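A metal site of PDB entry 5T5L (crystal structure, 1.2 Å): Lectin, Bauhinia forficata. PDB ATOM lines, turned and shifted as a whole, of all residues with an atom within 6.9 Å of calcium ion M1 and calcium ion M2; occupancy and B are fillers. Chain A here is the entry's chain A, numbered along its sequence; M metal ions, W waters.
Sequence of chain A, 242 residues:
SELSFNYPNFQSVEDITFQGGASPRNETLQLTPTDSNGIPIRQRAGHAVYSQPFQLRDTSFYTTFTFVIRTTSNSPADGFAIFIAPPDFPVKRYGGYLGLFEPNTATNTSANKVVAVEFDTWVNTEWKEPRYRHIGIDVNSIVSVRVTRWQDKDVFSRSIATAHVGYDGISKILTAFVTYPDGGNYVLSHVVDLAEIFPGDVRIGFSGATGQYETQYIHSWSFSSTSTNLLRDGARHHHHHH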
ATOM      1  N   ASP A  78      23.634  15.971  13.829  1.00  0.00           N
ATOM      2  CA  ASP A  78      23.284  15.354  15.088  1.00  0.00           C
ATOM      3  C   ASP A  78      22.778  13.922  15.006  1.00  0.00           C
ATOM      4  O   ASP A  78      22.681  13.260  16.061  1.00  0.00           O
ATOM      5  CB  ASP A  78      22.233  16.218  15.807  1.00  0.00           C
ATOM      6  CG  ASP A  78      22.889  17.368  16.521  1.00  0.00           C
ATOM      7  OD1 ASP A  78      23.362  17.132  17.684  1.00  0.00           O
ATOM      8  OD2 ASP A  78      23.046  18.459  15.938  1.00  0.00           O
ATOM      9  N   GLY A  95      19.571  20.655  15.894  1.00  0.00           N
ATOM     10  CA  GLY A  95      20.563  20.234  16.822  1.00  0.00           C
ATOM     11  C   GLY A  95      20.214  18.934  17.515  1.00  0.00           C
ATOM     12  O   GLY A  95      19.612  18.028  16.918  1.00  0.00           O
ATOM     13  N   GLY A  96      20.649  18.829  18.774  1.00  0.00           N
ATOM     14  CA  GLY A  96      20.551  17.546  19.470  1.00  0.00           C
ATOM     15  C   GLY A  96      19.149  17.106  19.788  1.00  0.00           C
ATOM     16  O   GLY A  96      18.921  15.965  20.188  1.00  0.00           O
ATOM     17  N   TYR A  97      18.171  17.995  19.597  1.00  0.00           N
ATOM     18  CA  TYR A  97      16.759  17.629  19.744  1.00  0.00           C
ATOM     19  C   TYR A  97      16.229  16.796  18.602  1.00  0.00           C
ATOM     20  O   TYR A  97      15.104  16.279  18.690  1.00  0.00           O
ATOM     21  CB  TYR A  97      15.932  18.906  19.881  1.00  0.00           C
ATOM     22  CG  TYR A  97      16.409  19.758  21.055  1.00  0.00           C
ATOM     23  CD1 TYR A  97      16.178  19.406  22.364  1.00  0.00           C
ATOM     24  CD2 TYR A  97      17.179  20.869  20.817  1.00  0.00           C
ATOM     25  CE1 TYR A  97      16.700  20.137  23.415  1.00  0.00           C
ATOM     26  CE2 TYR A  97      17.727  21.627  21.864  1.00  0.00           C
ATOM     27  CZ  TYR A  97      17.479  21.248  23.153  1.00  0.00           C
ATOM     28  OH  TYR A  97      17.990  21.986  24.199  1.00  0.00           O
ATOM     29  N   LEU A  98      17.029  16.635  17.524  1.00  0.00           N
ATOM     30  CA  LEU A  98      16.746  15.692  16.470  1.00  0.00           C
ATOM     31  C   LEU A  98      15.481  15.973  15.700  1.00  0.00           C
ATOM     32  O   LEU A  98      14.927  15.068  15.048  1.00  0.00           O
ATOM     33  CB  LEU A  98      16.832  14.228  16.933  1.00  0.00           C
ATOM     34  CG  LEU A  98      18.178  13.747  17.394  1.00  0.00           C
ATOM     35  CD1 LEU A  98      18.095  12.341  17.953  1.00  0.00           C
ATOM     36  CD2 LEU A  98      19.193  13.795  16.277  1.00  0.00           C
ATOM     37  N   GLU A 118      16.520   6.337  17.702  1.00  0.00           N
ATOM     38  CA  GLU A 118      17.468   7.374  17.295  1.00  0.00           C
ATOM     39  C   GLU A 118      18.806   6.784  16.988  1.00  0.00           C
ATOM     40  O   GLU A 118      19.280   5.816  17.602  1.00  0.00           O
ATOM     41  CB  GLU A 118      17.593   8.468  18.382  1.00  0.00           C
ATOM     42  CG  GLU A 118      18.195   8.000  19.686  1.00  0.00           C
ATOM     43  CD  GLU A 118      18.604   9.160  20.565  1.00  0.00           C
ATOM     44  OE1 GLU A 118      17.762  10.041  20.835  1.00  0.00           O
ATOM     45  OE2 GLU A 118      19.754   9.164  21.038  1.00  0.00           O
ATOM     46  N   PHE A 119      19.488   7.451  16.041  1.00  0.00           N
ATOM     47  CA  PHE A 119      20.844   7.184  15.595  1.00  0.00           C
ATOM     48  C   PHE A 119      21.607   8.471  15.843  1.00  0.00           C
ATOM     49  O   PHE A 119      21.472   9.441  15.095  1.00  0.00           O
ATOM     50  CB  PHE A 119      20.825   6.821  14.094  1.00  0.00           C
ATOM     51  CG  PHE A 119      20.020   5.587  13.791  1.00  0.00           C
ATOM     52  CD1 PHE A 119      18.611   5.665  13.730  1.00  0.00           C
ATOM     53  CD2 PHE A 119      20.626   4.374  13.537  1.00  0.00           C
ATOM     54  CE1 PHE A 119      17.875   4.525  13.503  1.00  0.00           C
ATOM     55  CE2 PHE A 119      19.868   3.233  13.275  1.00  0.00           C
ATOM     56  CZ  PHE A 119      18.502   3.312  13.262  1.00  0.00           C
ATOM     57  N   ASP A 120      22.323   8.517  16.962  1.00  0.00           N
ATOM     58  CA  ASP A 120      22.790   9.789  17.549  1.00  0.00           C
ATOM     59  C   ASP A 120      24.294   9.913  17.360  1.00  0.00           C
ATOM     60  O   ASP A 120      25.103   9.162  17.925  1.00  0.00           O
ATOM     61  CB  ASP A 120      22.390   9.813  19.037  1.00  0.00           C
ATOM     62  CG  ASP A 120      22.606  11.123  19.636  1.00  0.00           C
ATOM     63  OD1 ASP A 120      23.435  11.948  19.149  1.00  0.00           O
ATOM     64  OD2 ASP A 120      21.929  11.451  20.694  1.00  0.00           O
ATOM     65  N   THR A 121      24.702  10.888  16.511  1.00  0.00           N
ATOM     66  CA  THR A 121      26.095  11.073  16.142  1.00  0.00           C
ATOM     67  C   THR A 121      26.850  12.054  17.016  1.00  0.00           C
ATOM     68  O   THR A 121      28.068  12.181  16.810  1.00  0.00           O
ATOM     69  CB  THR A 121      26.219  11.534  14.673  1.00  0.00           C
ATOM     70  OG1 THR A 121      25.498  12.777  14.557  1.00  0.00           O
ATOM     71  CG2 THR A 121      25.645  10.528  13.674  1.00  0.00           C
ATOM     72  N   TRP A 122      26.180  12.765  17.923  1.00  0.00           N
ATOM     73  CA  TRP A 122      26.821  13.841  18.678  1.00  0.00           C
ATOM     74  C   TRP A 122      26.440  13.695  20.150  1.00  0.00           C
ATOM     75  O   TRP A 122      25.263  13.731  20.541  1.00  0.00           O
ATOM     76  CB  TRP A 122      26.361  15.226  18.149  1.00  0.00           C
ATOM     77  CG  TRP A 122      26.914  16.349  18.953  1.00  0.00           C
ATOM     78  CD1 TRP A 122      26.359  16.822  20.118  1.00  0.00           C
ATOM     79  CD2 TRP A 122      28.064  17.149  18.716  1.00  0.00           C
ATOM     80  NE1 TRP A 122      27.116  17.863  20.611  1.00  0.00           N
ATOM     81  CE2 TRP A 122      28.175  18.085  19.777  1.00  0.00           C
ATOM     82  CE3 TRP A 122      29.021  17.157  17.734  1.00  0.00           C
ATOM     83  CZ2 TRP A 122      29.203  19.026  19.845  1.00  0.00           C
ATOM     84  CZ3 TRP A 122      30.004  18.116  17.766  1.00  0.00           C
ATOM     85  CH2 TRP A 122      30.095  19.044  18.819  1.00  0.00           C
ATOM     86  N   VAL A 123      27.459  13.559  20.973  1.00  0.00           N
ATOM     87  CA  VAL A 123      27.282  13.396  22.407  1.00  0.00           C
ATOM     88  C   VAL A 123      26.929  14.776  23.040  1.00  0.00           C
ATOM     89  O   VAL A 123      27.772  15.671  23.113  1.00  0.00           O
ATOM     90  CB  VAL A 123      28.522  12.833  23.106  1.00  0.00           C
ATOM     91  CG1 VAL A 123      28.326  12.810  24.644  1.00  0.00           C
ATOM     92  CG2 VAL A 123      28.744  11.418  22.579  1.00  0.00           C
ATOM     93  N   ASN A 124      25.656  14.959  23.434  1.00  0.00           N
ATOM     94  CA  ASN A 124      25.240  16.226  24.036  1.00  0.00           C
ATOM     95  C   ASN A 124      25.609  16.257  25.492  1.00  0.00           C
ATOM     96  O   ASN A 124      25.401  15.320  26.214  1.00  0.00           O
ATOM     97  CB  ASN A 124      23.731  16.380  23.858  1.00  0.00           C
ATOM     98  CG  ASN A 124      23.396  16.793  22.427  1.00  0.00           C
ATOM     99  OD1 ASN A 124      23.165  15.896  21.556  1.00  0.00           O
ATOM    100  ND2 ASN A 124      23.466  18.058  22.132  1.00  0.00           N
ATOM    101  N   TRP A 127      21.977  17.349  28.323  1.00  0.00           N
ATOM    102  CA  TRP A 127      21.139  16.403  29.006  1.00  0.00           C
ATOM    103  C   TRP A 127      21.957  15.114  29.072  1.00  0.00           C
ATOM    104  O   TRP A 127      23.011  15.021  28.465  1.00  0.00           O
ATOM    105  CB  TRP A 127      19.799  16.137  28.293  1.00  0.00           C
ATOM    106  CG  TRP A 127      19.947  15.820  26.832  1.00  0.00           C
ATOM    107  CD1 TRP A 127      20.228  14.581  26.264  1.00  0.00           C
ATOM    108  CD2 TRP A 127      19.913  16.772  25.777  1.00  0.00           C
ATOM    109  NE1 TRP A 127      20.335  14.748  24.882  1.00  0.00           N
ATOM    110  CE2 TRP A 127      20.147  16.089  24.565  1.00  0.00           C
ATOM    111  CE3 TRP A 127      19.641  18.141  25.739  1.00  0.00           C
ATOM    112  CZ2 TRP A 127      20.088  16.722  23.334  1.00  0.00           C
ATOM    113  CZ3 TRP A 127      19.615  18.766  24.503  1.00  0.00           C
ATOM    114  CH2 TRP A 127      19.863  18.069  23.323  1.00  0.00           C
ATOM    115  N   LYS A 128      21.437  14.169  29.829  1.00  0.00           N
ATOM    116  CA  LYS A 128      22.172  12.923  30.017  1.00  0.00           C
ATOM    117  C   LYS A 128      22.158  12.074  28.749  1.00  0.00           C
ATOM    118  O   LYS A 128      21.100  11.707  28.246  1.00  0.00           O
ATOM    119  CB  LYS A 128      21.477  12.085  31.118  1.00  0.00           C
ATOM    120  CG  LYS A 128      22.141  10.750  31.399  1.00  0.00           C
ATOM    121  CD  LYS A 128      21.702  10.063  32.670  1.00  0.00           C
ATOM    122  CE  LYS A 128      20.321   9.440  32.528  1.00  0.00           C
ATOM    123  NZ  LYS A 128      20.269   8.216  31.658  1.00  0.00           N
ATOM    124  N   GLU A 129      23.325  11.717  28.275  1.00  0.00           N
ATOM    125  CA  GLU A 129      23.441  10.666  27.280  1.00  0.00           C
ATOM    126  C   GLU A 129      24.840  10.057  27.322  1.00  0.00           C
ATOM    127  O   GLU A 129      25.680  10.523  28.090  1.00  0.00           O
ATOM    128  CB  GLU A 129      22.864  11.089  25.911  1.00  0.00           C
ATOM    129  CG  GLU A 129      23.403  12.369  25.298  1.00  0.00           C
ATOM    130  CD  GLU A 129      22.914  12.515  23.885  1.00  0.00           C
ATOM    131  OE1 GLU A 129      21.796  12.056  23.709  1.00  0.00           O
ATOM    132  OE2 GLU A 129      23.617  13.017  23.011  1.00  0.00           O
ATOM    133  N   PRO A 130      24.976   8.846  26.811  1.00  0.00           N
ATOM    134  CA  PRO A 130      26.252   8.151  26.930  1.00  0.00           C
ATOM    135  C   PRO A 130      27.404   8.959  26.342  1.00  0.00           C
ATOM    136  O   PRO A 130      27.198   9.718  25.458  1.00  0.00           O
ATOM    137  CB  PRO A 130      26.035   6.860  26.182  1.00  0.00           C
ATOM    138  CG  PRO A 130      24.743   6.883  25.605  1.00  0.00           C
ATOM    139  CD  PRO A 130      24.016   8.117  25.956  1.00  0.00           C
ATOM    140  N   HIS A 134      25.656   6.611  19.728  1.00  0.00           N
ATOM    141  CA  HIS A 134      24.772   5.594  20.265  1.00  0.00           C
ATOM    142  C   HIS A 134      23.499   5.502  19.444  1.00  0.00           C
ATOM    143  O   HIS A 134      23.107   6.454  18.774  1.00  0.00           O
ATOM    144  CB  HIS A 134      24.438   5.880  21.757  1.00  0.00           C
ATOM    145  CG  HIS A 134      23.944   7.267  22.009  1.00  0.00           C
ATOM    146  ND1 HIS A 134      24.798   8.351  22.159  1.00  0.00           N
ATOM    147  CD2 HIS A 134      22.690   7.788  22.130  1.00  0.00           C
ATOM    148  CE1 HIS A 134      24.070   9.440  22.385  1.00  0.00           C
ATOM    149  NE2 HIS A 134      22.792   9.124  22.349  1.00  0.00           N
ATOM    150  N   GLY A 136      19.430   4.526  20.253  1.00  0.00           N
ATOM    151  CA  GLY A 136      18.557   4.488  21.418  1.00  0.00           C
ATOM    152  C   GLY A 136      17.102   4.411  21.086  1.00  0.00           C
ATOM    153  O   GLY A 136      16.678   4.727  19.983  1.00  0.00           O
ATOM    154  N   ASP A 138      13.676   6.106  22.382  1.00  0.00           N
ATOM    155  CA  ASP A 138      13.198   7.290  23.086  1.00  0.00           C
ATOM    156  C   ASP A 138      11.700   7.188  23.251  1.00  0.00           C
ATOM    157  O   ASP A 138      10.972   6.905  22.314  1.00  0.00           O
ATOM    158  CB  ASP A 138      13.516   8.559  22.249  1.00  0.00           C
ATOM    159  CG  ASP A 138      14.969   8.780  22.001  1.00  0.00           C
ATOM    160  OD1 ASP A 138      15.825   8.197  22.680  1.00  0.00           O
ATOM    161  OD2 ASP A 138      15.258   9.595  21.042  1.00  0.00           O
ATOM    162  N   ILE A 142      14.171  13.140  25.056  1.00  0.00           N
ATOM    163  CA  ILE A 142      15.449  13.012  24.331  1.00  0.00           C
ATOM    164  C   ILE A 142      16.483  12.199  25.116  1.00  0.00           C
ATOM    165  O   ILE A 142      17.502  11.802  24.566  1.00  0.00           O
ATOM    166  CB  ILE A 142      15.996  14.434  23.959  1.00  0.00           C
ATOM    167  CG1 ILE A 142      17.039  14.436  22.835  1.00  0.00           C
ATOM    168  CG2 ILE A 142      16.501  15.195  25.188  1.00  0.00           C
ATOM    169  CD1 ILE A 142      16.627  13.804  21.492  1.00  0.00           C
ATOM    170  N   VAL A 143      16.207  11.923  26.391  1.00  0.00           N
ATOM    171  CA  VAL A 143      17.050  11.041  27.205  1.00  0.00           C
ATOM    172  C   VAL A 143      16.535   9.628  26.997  1.00  0.00           C
ATOM    173  O   VAL A 143      15.456   9.256  27.500  1.00  0.00           O
ATOM    174  CB  VAL A 143      17.053  11.437  28.687  1.00  0.00           C
ATOM    175  CG1 VAL A 143      17.868  10.427  29.493  1.00  0.00           C
ATOM    176  CG2 VAL A 143      17.669  12.839  28.861  1.00  0.00           C
ATOM    177  N   SER A 144      17.248   8.827  26.224  1.00  0.00           N
ATOM    178  CA  SER A 144      16.759   7.502  25.816  1.00  0.00           C
ATOM    179  C   SER A 144      16.487   6.600  27.023  1.00  0.00           C
ATOM    180  O   SER A 144      17.219   6.577  27.997  1.00  0.00           O
ATOM    181  CB  SER A 144      17.806   6.846  24.931  1.00  0.00           C
ATOM    182  OG  SER A 144      18.161   7.585  23.799  1.00  0.00           O
ATOM    183  N   VAL A 147      19.656   2.413  25.515  1.00  0.00           N
ATOM    184  CA  VAL A 147      20.665   2.975  24.657  1.00  0.00           C
ATOM    185  C   VAL A 147      21.864   2.082  24.585  1.00  0.00           C
ATOM    186  O   VAL A 147      22.272   1.498  25.656  1.00  0.00           O
ATOM    187  CB  VAL A 147      20.970   4.444  25.134  1.00  0.00           C
ATOM    188  CG1 VAL A 147      21.702   4.472  26.518  1.00  0.00           C
ATOM    189  CG2 VAL A 147      21.706   5.239  24.105  1.00  0.00           C
HETATM  190 CA    CA M   1      20.957  10.491  22.347  1.00  0.00          CA
HETATM  191 CA    CA M   2      22.956  13.692  20.812  1.00  0.00          CA
HETATM  192  O   HOH W   1      22.711  14.675  18.655  1.00  0.00           O
HETATM  193  O   HOH W   2      19.142  11.784  22.273  1.00  0.00           O
HETATM  194  O   HOH W   3      20.610  14.020  21.183  1.00  0.00           O
HETATM  195  O   HOH W   4      20.251   9.292  24.002  1.00  0.00           O
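O of Gly 136 is in hydrogen-bond range of N of Glu 118 (2.8 Å). The side-chain carboxylate of Glu 118 sits close to the side-chain carboxylate of Asp 138, 2.6 Å away. NE1 of Trp 127 lies close to OE1 of Glu 129 (3.3 Å).
Within 4 Å of calcium ion M1: Glu 118, Asp 120, Glu 129 and His 134.
Four residues have an atom within 4 Å of calcium ion M2: Asp 120, Trp 122, Asn 124 and Glu 129. The nearest printed residue that does not touch calcium ion M2 is Val 123 (4.5 Å).
Calcium ion M1 is bound by OD2 of Asp 120 (2.1 Å), water W4 (2.2 Å), OE2 of Glu 118 (2.2 Å), water W2 (2.2 Å), OE1 of Glu 129 (2.2 Å) and NE2 of His 134 (2.3 Å).
Calcium ion M2 is bound by O of Trp 122 (2.3 Å), OD1 of Asn 124 (2.3 Å), water W1 (2.4 Å), OE2 of Glu 129 (2.4 Å), water W3 (2.4 Å), OD1 of Asp 120 (2.5 Å) and OD2 of Asp 120 (2.5 Å). Calcium ion M2 has seven donor atoms within binding distance.
Water W2 bridges the side-chain carboxylate of Glu 118 (2.6 Å) and the backbone carbonyl oxygen of Ile 142 (2.8 Å).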
